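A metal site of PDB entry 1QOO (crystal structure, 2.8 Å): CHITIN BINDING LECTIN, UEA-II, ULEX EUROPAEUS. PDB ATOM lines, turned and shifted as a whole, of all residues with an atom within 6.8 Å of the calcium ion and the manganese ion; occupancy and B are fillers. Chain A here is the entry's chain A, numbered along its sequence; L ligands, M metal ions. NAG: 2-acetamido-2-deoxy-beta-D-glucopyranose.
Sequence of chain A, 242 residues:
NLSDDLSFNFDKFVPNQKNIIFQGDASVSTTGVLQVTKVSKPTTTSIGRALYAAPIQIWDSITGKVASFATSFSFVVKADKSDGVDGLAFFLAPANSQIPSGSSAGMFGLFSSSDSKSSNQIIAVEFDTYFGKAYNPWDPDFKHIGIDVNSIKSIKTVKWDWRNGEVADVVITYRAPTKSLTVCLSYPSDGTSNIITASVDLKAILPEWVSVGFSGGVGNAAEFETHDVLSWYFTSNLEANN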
ATOM      1  N   ASP A  86     -33.211 -29.435 -10.081  1.00  0.00           N
ATOM      2  CA  ASP A  86     -32.097 -28.504 -10.172  1.00  0.00           C
ATOM      3  C   ASP A  86     -31.148 -28.645  -8.981  1.00  0.00           C
ATOM      4  O   ASP A  86     -29.970 -28.294  -9.077  1.00  0.00           O
ATOM      5  CB  ASP A  86     -32.646 -27.078 -10.150  1.00  0.00           C
ATOM      6  CG  ASP A  86     -32.633 -26.449 -11.514  1.00  0.00           C
ATOM      7  OD1 ASP A  86     -33.615 -26.625 -12.250  1.00  0.00           O
ATOM      8  OD2 ASP A  86     -31.628 -25.781 -11.830  1.00  0.00           O
ATOM      9  N   GLY A  87     -31.677 -29.102  -7.860  1.00  0.00           N
ATOM     10  CA  GLY A  87     -30.854 -29.262  -6.680  1.00  0.00           C
ATOM     11  C   GLY A  87     -31.615 -28.991  -5.402  1.00  0.00           C
ATOM     12  O   GLY A  87     -32.806 -28.663  -5.412  1.00  0.00           O
ATOM     13  N   ALA A 105     -36.043 -22.021 -10.132  1.00  0.00           N
ATOM     14  CA  ALA A 105     -35.557 -23.284  -9.594  1.00  0.00           C
ATOM     15  C   ALA A 105     -34.036 -23.307  -9.455  1.00  0.00           C
ATOM     16  O   ALA A 105     -33.501 -23.822  -8.465  1.00  0.00           O
ATOM     17  CB  ALA A 105     -36.024 -24.423 -10.468  1.00  0.00           C
ATOM     18  N   GLY A 106     -33.350 -22.711 -10.420  1.00  0.00           N
ATOM     19  CA  GLY A 106     -31.898 -22.670 -10.397  1.00  0.00           C
ATOM     20  C   GLY A 106     -31.320 -21.845  -9.280  1.00  0.00           C
ATOM     21  O   GLY A 106     -30.100 -21.867  -9.038  1.00  0.00           O
ATOM     22  N   MET A 107     -32.175 -21.067  -8.619  1.00  0.00           N
ATOM     23  CA  MET A 107     -31.767 -20.242  -7.494  1.00  0.00           C
ATOM     24  C   MET A 107     -32.353 -20.788  -6.194  1.00  0.00           C
ATOM     25  O   MET A 107     -32.267 -20.165  -5.135  1.00  0.00           O
ATOM     26  CB  MET A 107     -32.134 -18.789  -7.738  1.00  0.00           C
ATOM     27  CG  MET A 107     -31.406 -18.246  -8.940  1.00  0.00           C
ATOM     28  SD  MET A 107     -31.663 -16.526  -9.269  1.00  0.00           S
ATOM     29  CE  MET A 107     -33.335 -16.531  -9.961  1.00  0.00           C
ATOM     30  N   PHE A 108     -32.954 -21.977  -6.305  1.00  0.00           N
ATOM     31  CA  PHE A 108     -33.543 -22.709  -5.177  1.00  0.00           C
ATOM     32  C   PHE A 108     -34.523 -21.906  -4.336  1.00  0.00           C
ATOM     33  O   PHE A 108     -34.657 -22.160  -3.136  1.00  0.00           O
ATOM     34  CB  PHE A 108     -32.418 -23.258  -4.297  1.00  0.00           C
ATOM     35  CG  PHE A 108     -31.327 -23.960  -5.063  1.00  0.00           C
ATOM     36  CD1 PHE A 108     -31.593 -25.115  -5.800  1.00  0.00           C
ATOM     37  CD2 PHE A 108     -30.025 -23.447  -5.069  1.00  0.00           C
ATOM     38  CE1 PHE A 108     -30.584 -25.746  -6.528  1.00  0.00           C
ATOM     39  CE2 PHE A 108     -29.007 -24.084  -5.800  1.00  0.00           C
ATOM     40  CZ  PHE A 108     -29.282 -25.237  -6.525  1.00  0.00           C
ATOM     41  N   GLU A 126     -25.551 -25.579  -1.009  1.00  0.00           N
ATOM     42  CA  GLU A 126     -26.284 -26.156  -2.116  1.00  0.00           C
ATOM     43  C   GLU A 126     -25.735 -27.475  -2.611  1.00  0.00           C
ATOM     44  O   GLU A 126     -24.533 -27.728  -2.560  1.00  0.00           O
ATOM     45  CB  GLU A 126     -26.324 -25.166  -3.293  1.00  0.00           C
ATOM     46  CG  GLU A 126     -24.961 -24.712  -3.785  1.00  0.00           C
ATOM     47  CD  GLU A 126     -24.998 -24.086  -5.162  1.00  0.00           C
ATOM     48  OE1 GLU A 126     -25.665 -23.042  -5.328  1.00  0.00           O
ATOM     49  OE2 GLU A 126     -24.370 -24.632  -6.090  1.00  0.00           O
ATOM     50  N   ASP A 128     -26.155 -28.829  -5.876  1.00  0.00           N
ATOM     51  CA  ASP A 128     -26.499 -28.464  -7.256  1.00  0.00           C
ATOM     52  C   ASP A 128     -26.342 -29.578  -8.281  1.00  0.00           C
ATOM     53  O   ASP A 128     -25.227 -30.009  -8.571  1.00  0.00           O
ATOM     54  CB  ASP A 128     -25.589 -27.295  -7.632  1.00  0.00           C
ATOM     55  CG  ASP A 128     -26.196 -26.360  -8.638  1.00  0.00           C
ATOM     56  OD1 ASP A 128     -27.102 -26.777  -9.404  1.00  0.00           O
ATOM     57  OD2 ASP A 128     -25.730 -25.200  -8.682  1.00  0.00           O
ATOM     58  N   THR A 129     -27.455 -29.996  -8.868  1.00  0.00           N
ATOM     59  CA  THR A 129     -27.422 -31.071  -9.869  1.00  0.00           C
ATOM     60  C   THR A 129     -27.366 -30.574 -11.306  1.00  0.00           C
ATOM     61  O   THR A 129     -26.983 -31.317 -12.210  1.00  0.00           O
ATOM     62  CB  THR A 129     -28.643 -31.979  -9.739  1.00  0.00           C
ATOM     63  OG1 THR A 129     -29.822 -31.188  -9.812  1.00  0.00           O
ATOM     64  CG2 THR A 129     -28.611 -32.747  -8.430  1.00  0.00           C
ATOM     65  N   TYR A 130     -27.810 -29.342 -11.533  1.00  0.00           N
ATOM     66  CA  TYR A 130     -27.790 -28.753 -12.870  1.00  0.00           C
ATOM     67  C   TYR A 130     -26.736 -27.653 -12.958  1.00  0.00           C
ATOM     68  O   TYR A 130     -26.725 -26.705 -12.159  1.00  0.00           O
ATOM     69  CB  TYR A 130     -29.181 -28.201 -13.225  1.00  0.00           C
ATOM     70  CG  TYR A 130     -29.232 -27.504 -14.574  1.00  0.00           C
ATOM     71  CD1 TYR A 130     -29.296 -28.235 -15.762  1.00  0.00           C
ATOM     72  CD2 TYR A 130     -29.191 -26.111 -14.662  1.00  0.00           C
ATOM     73  CE1 TYR A 130     -29.319 -27.588 -17.001  1.00  0.00           C
ATOM     74  CE2 TYR A 130     -29.209 -25.455 -15.897  1.00  0.00           C
ATOM     75  CZ  TYR A 130     -29.274 -26.198 -17.058  1.00  0.00           C
ATOM     76  OH  TYR A 130     -29.265 -25.539 -18.280  1.00  0.00           O
ATOM     77  N   PHE A 131     -25.875 -27.765 -13.956  1.00  0.00           N
ATOM     78  CA  PHE A 131     -24.817 -26.796 -14.150  1.00  0.00           C
ATOM     79  C   PHE A 131     -24.747 -26.291 -15.595  1.00  0.00           C
ATOM     80  O   PHE A 131     -23.712 -25.764 -16.032  1.00  0.00           O
ATOM     81  CB  PHE A 131     -23.484 -27.416 -13.726  1.00  0.00           C
ATOM     82  CG  PHE A 131     -23.179 -28.716 -14.424  1.00  0.00           C
ATOM     83  CD1 PHE A 131     -23.617 -29.929 -13.905  1.00  0.00           C
ATOM     84  CD2 PHE A 131     -22.460 -28.728 -15.610  1.00  0.00           C
ATOM     85  CE1 PHE A 131     -23.344 -31.135 -14.544  1.00  0.00           C
ATOM     86  CE2 PHE A 131     -22.178 -29.932 -16.270  1.00  0.00           C
ATOM     87  CZ  PHE A 131     -22.620 -31.135 -15.736  1.00  0.00           C
ATOM     88  N   GLY A 132     -25.835 -26.450 -16.337  1.00  0.00           N
ATOM     89  CA  GLY A 132     -25.871 -26.017 -17.727  1.00  0.00           C
ATOM     90  C   GLY A 132     -25.558 -24.549 -17.909  1.00  0.00           C
ATOM     91  O   GLY A 132     -26.230 -23.685 -17.361  1.00  0.00           O
ATOM     92  N   ASN A 136     -27.513 -21.566 -16.042  1.00  0.00           N
ATOM     93  CA  ASN A 136     -26.730 -21.282 -14.836  1.00  0.00           C
ATOM     94  C   ASN A 136     -25.271 -20.999 -15.200  1.00  0.00           C
ATOM     95  O   ASN A 136     -24.370 -21.784 -14.861  1.00  0.00           O
ATOM     96  CB  ASN A 136     -26.738 -22.470 -13.857  1.00  0.00           C
ATOM     97  CG  ASN A 136     -28.125 -22.851 -13.390  1.00  0.00           C
ATOM     98  OD1 ASN A 136     -28.307 -23.947 -12.863  1.00  0.00           O
ATOM     99  ND2 ASN A 136     -29.090 -21.965 -13.550  1.00  0.00           N
ATOM    100  N   TRP A 138     -23.162 -19.225 -13.889  1.00  0.00           N
ATOM    101  CA  TRP A 138     -22.327 -19.078 -12.694  1.00  0.00           C
ATOM    102  C   TRP A 138     -21.771 -20.393 -12.131  1.00  0.00           C
ATOM    103  O   TRP A 138     -20.854 -20.375 -11.309  1.00  0.00           O
ATOM    104  CB  TRP A 138     -23.151 -18.395 -11.607  1.00  0.00           C
ATOM    105  CG  TRP A 138     -24.445 -19.119 -11.340  1.00  0.00           C
ATOM    106  CD1 TRP A 138     -24.620 -20.256 -10.603  1.00  0.00           C
ATOM    107  CD2 TRP A 138     -25.735 -18.761 -11.847  1.00  0.00           C
ATOM    108  NE1 TRP A 138     -25.939 -20.634 -10.629  1.00  0.00           N
ATOM    109  CE2 TRP A 138     -26.646 -19.743 -11.385  1.00  0.00           C
ATOM    110  CE3 TRP A 138     -26.213 -17.717 -12.645  1.00  0.00           C
ATOM    111  CZ2 TRP A 138     -28.009 -19.705 -11.698  1.00  0.00           C
ATOM    112  CZ3 TRP A 138     -27.580 -17.688 -12.962  1.00  0.00           C
ATOM    113  CH2 TRP A 138     -28.456 -18.674 -12.479  1.00  0.00           C
ATOM    114  N   ASP A 139     -22.350 -21.525 -12.531  1.00  0.00           N
ATOM    115  CA  ASP A 139     -21.946 -22.840 -12.048  1.00  0.00           C
ATOM    116  C   ASP A 139     -20.716 -23.417 -12.718  1.00  0.00           C
ATOM    117  O   ASP A 139     -20.393 -23.046 -13.845  1.00  0.00           O
ATOM    118  CB  ASP A 139     -23.099 -23.846 -12.257  1.00  0.00           C
ATOM    119  CG  ASP A 139     -24.138 -23.811 -11.143  1.00  0.00           C
ATOM    120  OD1 ASP A 139     -23.779 -23.490  -9.984  1.00  0.00           O
ATOM    121  OD2 ASP A 139     -25.320 -24.140 -11.427  1.00  0.00           O
ATOM    122  N   PRO A 140     -19.966 -24.280 -12.004  1.00  0.00           N
ATOM    123  CA  PRO A 140     -18.762 -24.937 -12.534  1.00  0.00           C
ATOM    124  C   PRO A 140     -19.238 -26.081 -13.443  1.00  0.00           C
ATOM    125  O   PRO A 140     -20.445 -26.374 -13.476  1.00  0.00           O
ATOM    126  CB  PRO A 140     -18.057 -25.440 -11.278  1.00  0.00           C
ATOM    127  CG  PRO A 140     -19.180 -25.679 -10.340  1.00  0.00           C
ATOM    128  CD  PRO A 140     -20.041 -24.468 -10.540  1.00  0.00           C
ATOM    129  N   HIS A 144     -22.184 -30.193  -8.079  1.00  0.00           N
ATOM    130  CA  HIS A 144     -21.361 -29.730  -6.973  1.00  0.00           C
ATOM    131  C   HIS A 144     -22.050 -29.424  -5.646  1.00  0.00           C
ATOM    132  O   HIS A 144     -23.278 -29.356  -5.568  1.00  0.00           O
ATOM    133  CB  HIS A 144     -20.643 -28.459  -7.441  1.00  0.00           C
ATOM    134  CG  HIS A 144     -21.588 -27.431  -8.007  1.00  0.00           C
ATOM    135  ND1 HIS A 144     -22.139 -27.538  -9.257  1.00  0.00           N
ATOM    136  CD2 HIS A 144     -22.114 -26.307  -7.460  1.00  0.00           C
ATOM    137  CE1 HIS A 144     -22.974 -26.538  -9.465  1.00  0.00           C
ATOM    138  NE2 HIS A 144     -22.980 -25.767  -8.392  1.00  0.00           N
ATOM    139  N   ILE A 145     -21.226 -29.259  -4.627  1.00  0.00           N
ATOM    140  CA  ILE A 145     -21.678 -28.844  -3.306  1.00  0.00           C
ATOM    141  C   ILE A 145     -21.090 -27.444  -3.241  1.00  0.00           C
ATOM    142  O   ILE A 145     -19.908 -27.253  -3.550  1.00  0.00           O
ATOM    143  CB  ILE A 145     -21.062 -29.676  -2.173  1.00  0.00           C
ATOM    144  CG1 ILE A 145     -21.460 -31.145  -2.316  1.00  0.00           C
ATOM    145  CG2 ILE A 145     -21.517 -29.121  -0.829  1.00  0.00           C
ATOM    146  CD1 ILE A 145     -20.815 -32.036  -1.292  1.00  0.00           C
ATOM    147  N   GLY A 146     -21.900 -26.459  -2.906  1.00  0.00           N
ATOM    148  CA  GLY A 146     -21.381 -25.101  -2.847  1.00  0.00           C
ATOM    149  C   GLY A 146     -21.809 -24.343  -1.615  1.00  0.00           C
ATOM    150  O   GLY A 146     -22.873 -24.599  -1.049  1.00  0.00           O
ATOM    151  N   ASP A 148     -22.891 -20.881  -0.434  1.00  0.00           N
ATOM    152  CA  ASP A 148     -23.424 -19.650  -1.007  1.00  0.00           C
ATOM    153  C   ASP A 148     -23.560 -18.568   0.037  1.00  0.00           C
ATOM    154  O   ASP A 148     -24.167 -18.779   1.094  1.00  0.00           O
ATOM    155  CB  ASP A 148     -24.776 -19.912  -1.656  1.00  0.00           C
ATOM    156  CG  ASP A 148     -24.709 -20.917  -2.789  1.00  0.00           C
ATOM    157  OD1 ASP A 148     -23.603 -21.359  -3.160  1.00  0.00           O
ATOM    158  OD2 ASP A 148     -25.774 -21.261  -3.325  1.00  0.00           O
ATOM    159  N   ILE A 152     -26.065 -16.758  -5.601  1.00  0.00           N
ATOM    160  CA  ILE A 152     -26.187 -18.100  -6.151  1.00  0.00           C
ATOM    161  C   ILE A 152     -24.863 -18.564  -6.752  1.00  0.00           C
ATOM    162  O   ILE A 152     -24.701 -19.731  -7.119  1.00  0.00           O
ATOM    163  CB  ILE A 152     -27.329 -18.162  -7.200  1.00  0.00           C
ATOM    164  CG1 ILE A 152     -27.694 -19.615  -7.519  1.00  0.00           C
ATOM    165  CG2 ILE A 152     -26.936 -17.414  -8.444  1.00  0.00           C
ATOM    166  CD1 ILE A 152     -28.157 -20.436  -6.327  1.00  0.00           C
ATOM    167  N   LYS A 153     -23.923 -17.631  -6.867  1.00  0.00           N
ATOM    168  CA  LYS A 153     -22.591 -17.917  -7.375  1.00  0.00           C
ATOM    169  C   LYS A 153     -21.761 -18.222  -6.124  1.00  0.00           C
ATOM    170  O   LYS A 153     -21.335 -17.324  -5.411  1.00  0.00           O
ATOM    171  CB  LYS A 153     -22.041 -16.707  -8.141  1.00  0.00           C
ATOM    172  CG  LYS A 153     -20.614 -16.866  -8.672  1.00  0.00           C
ATOM    173  CD  LYS A 153     -20.220 -15.661  -9.529  1.00  0.00           C
ATOM    174  CE  LYS A 153     -18.725 -15.565  -9.730  1.00  0.00           C
ATOM    175  NZ  LYS A 153     -18.169 -16.840 -10.251  1.00  0.00           N
ATOM    176  N   SER A 154     -21.602 -19.514  -5.851  1.00  0.00           N
ATOM    177  CA  SER A 154     -20.883 -20.026  -4.685  1.00  0.00           C
ATOM    178  C   SER A 154     -19.489 -19.437  -4.530  1.00  0.00           C
ATOM    179  O   SER A 154     -18.809 -19.174  -5.521  1.00  0.00           O
ATOM    180  CB  SER A 154     -20.759 -21.540  -4.782  1.00  0.00           C
ATOM    181  OG  SER A 154     -21.966 -22.144  -5.231  1.00  0.00           O
ATOM    182  N   THR A 157     -16.709 -24.253  -4.183  1.00  0.00           N
ATOM    183  CA  THR A 157     -17.434 -25.444  -4.588  1.00  0.00           C
ATOM    184  C   THR A 157     -16.505 -26.645  -4.598  1.00  0.00           C
ATOM    185  O   THR A 157     -15.295 -26.505  -4.497  1.00  0.00           O
ATOM    186  CB  THR A 157     -18.047 -25.319  -6.015  1.00  0.00           C
ATOM    187  OG1 THR A 157     -17.002 -25.222  -6.979  1.00  0.00           O
ATOM    188  CG2 THR A 157     -18.931 -24.099  -6.115  1.00  0.00           C
HETATM  189  C1  NAG L   1     -35.284 -23.281 -16.256  1.00  0.00           C
HETATM  190  C2  NAG L   1     -35.333 -22.447 -14.975  1.00  0.00           C
HETATM  191  C3  NAG L   1     -33.942 -22.346 -14.347  1.00  0.00           C
HETATM  192  C4  NAG L   1     -33.344 -23.744 -14.184  1.00  0.00           C
HETATM  193  C5  NAG L   1     -33.362 -24.462 -15.527  1.00  0.00           C
HETATM  194  C6  NAG L   1     -32.781 -25.851 -15.479  1.00  0.00           C
HETATM  195  C7  NAG L   1     -37.150 -20.867 -15.143  1.00  0.00           C
HETATM  196  C8  NAG L   1     -37.609 -19.463 -15.495  1.00  0.00           C
HETATM  197  N2  NAG L   1     -35.853 -21.129 -15.298  1.00  0.00           N
HETATM  198  O1  NAG L   1     -36.572 -23.482 -16.727  1.00  0.00           O
HETATM  199  O3  NAG L   1     -34.021 -21.704 -13.068  1.00  0.00           O
HETATM  200  O4  NAG L   1     -31.976 -23.641 -13.739  1.00  0.00           O
HETATM  201  O5  NAG L   1     -34.713 -24.566 -15.994  1.00  0.00           O
HETATM  202  O6  NAG L   1     -33.721 -26.767 -14.927  1.00  0.00           O
HETATM  203  O7  NAG L   1     -37.961 -21.704 -14.729  1.00  0.00           O
HETATM  204 CA    CA M   1     -27.664 -24.902 -10.690  1.00  0.00          CA
HETATM  205 MN    MN M   2     -24.068 -23.964  -8.025  1.00  0.00          MN
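Residues that only touch the manganese ion: Ser 154 (3.9 Å).
Of the 24 residues printed, 4 come within 4 Å of the calcium ion.
The nearest printed residue that does not touch the calcium ion is Asp 86 (4.2 Å).
The backbone carbonyl oxygen (O) of Asp 86 is in hydrogen-bond range of the backbone NH (N) of Tyr 130, at 3.4 Å.
OE1 of Glu 126 sits close to OD2 of Asp 148, 2.7 Å away.
N of Glu 126 lies within hydrogen-bond range of O of Gly 146, 2.9 Å away.
OD1 of Asp 148 is in hydrogen-bond range of OG of Ser 154 (2.8 Å).
The calcium ion is bound by OD1 of Asp 128, at 2.3 Å.
OD1 of Asn 136 is bound to the calcium ion, 2.5 Å away.
O of Tyr 130 is bound to the calcium ion, 2.5 Å away.
The calcium ion is bound by OD2 of Asp 139, 2.6 Å away.
The calcium ion is bound by OD2 of Asp 128 (2.8 Å).
The manganese ion is bound by OD1 of Asp 139 (2.0 Å).
The manganese ion is bound by OE2 of Glu 126, at 2.1 Å.
NE2 of His 144 is bound to the manganese ion, at 2.1 Å.
OD2 of Asp 128 binds the manganese ion (2.2 Å).
The manganese ion has four donor atoms within binding distance.
An oxygen (O3) of the ligand lies within hydrogen-bond range of the backbone NH (N) of Gly 106.
The side-chain carboxylate of Asp 86 sits at hydrogen-bond distance from an oxygen (O6) of the ligand.
ND2 of Asn 136 lies within hydrogen-bond range of O4 of the ligand (3.3 Å).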
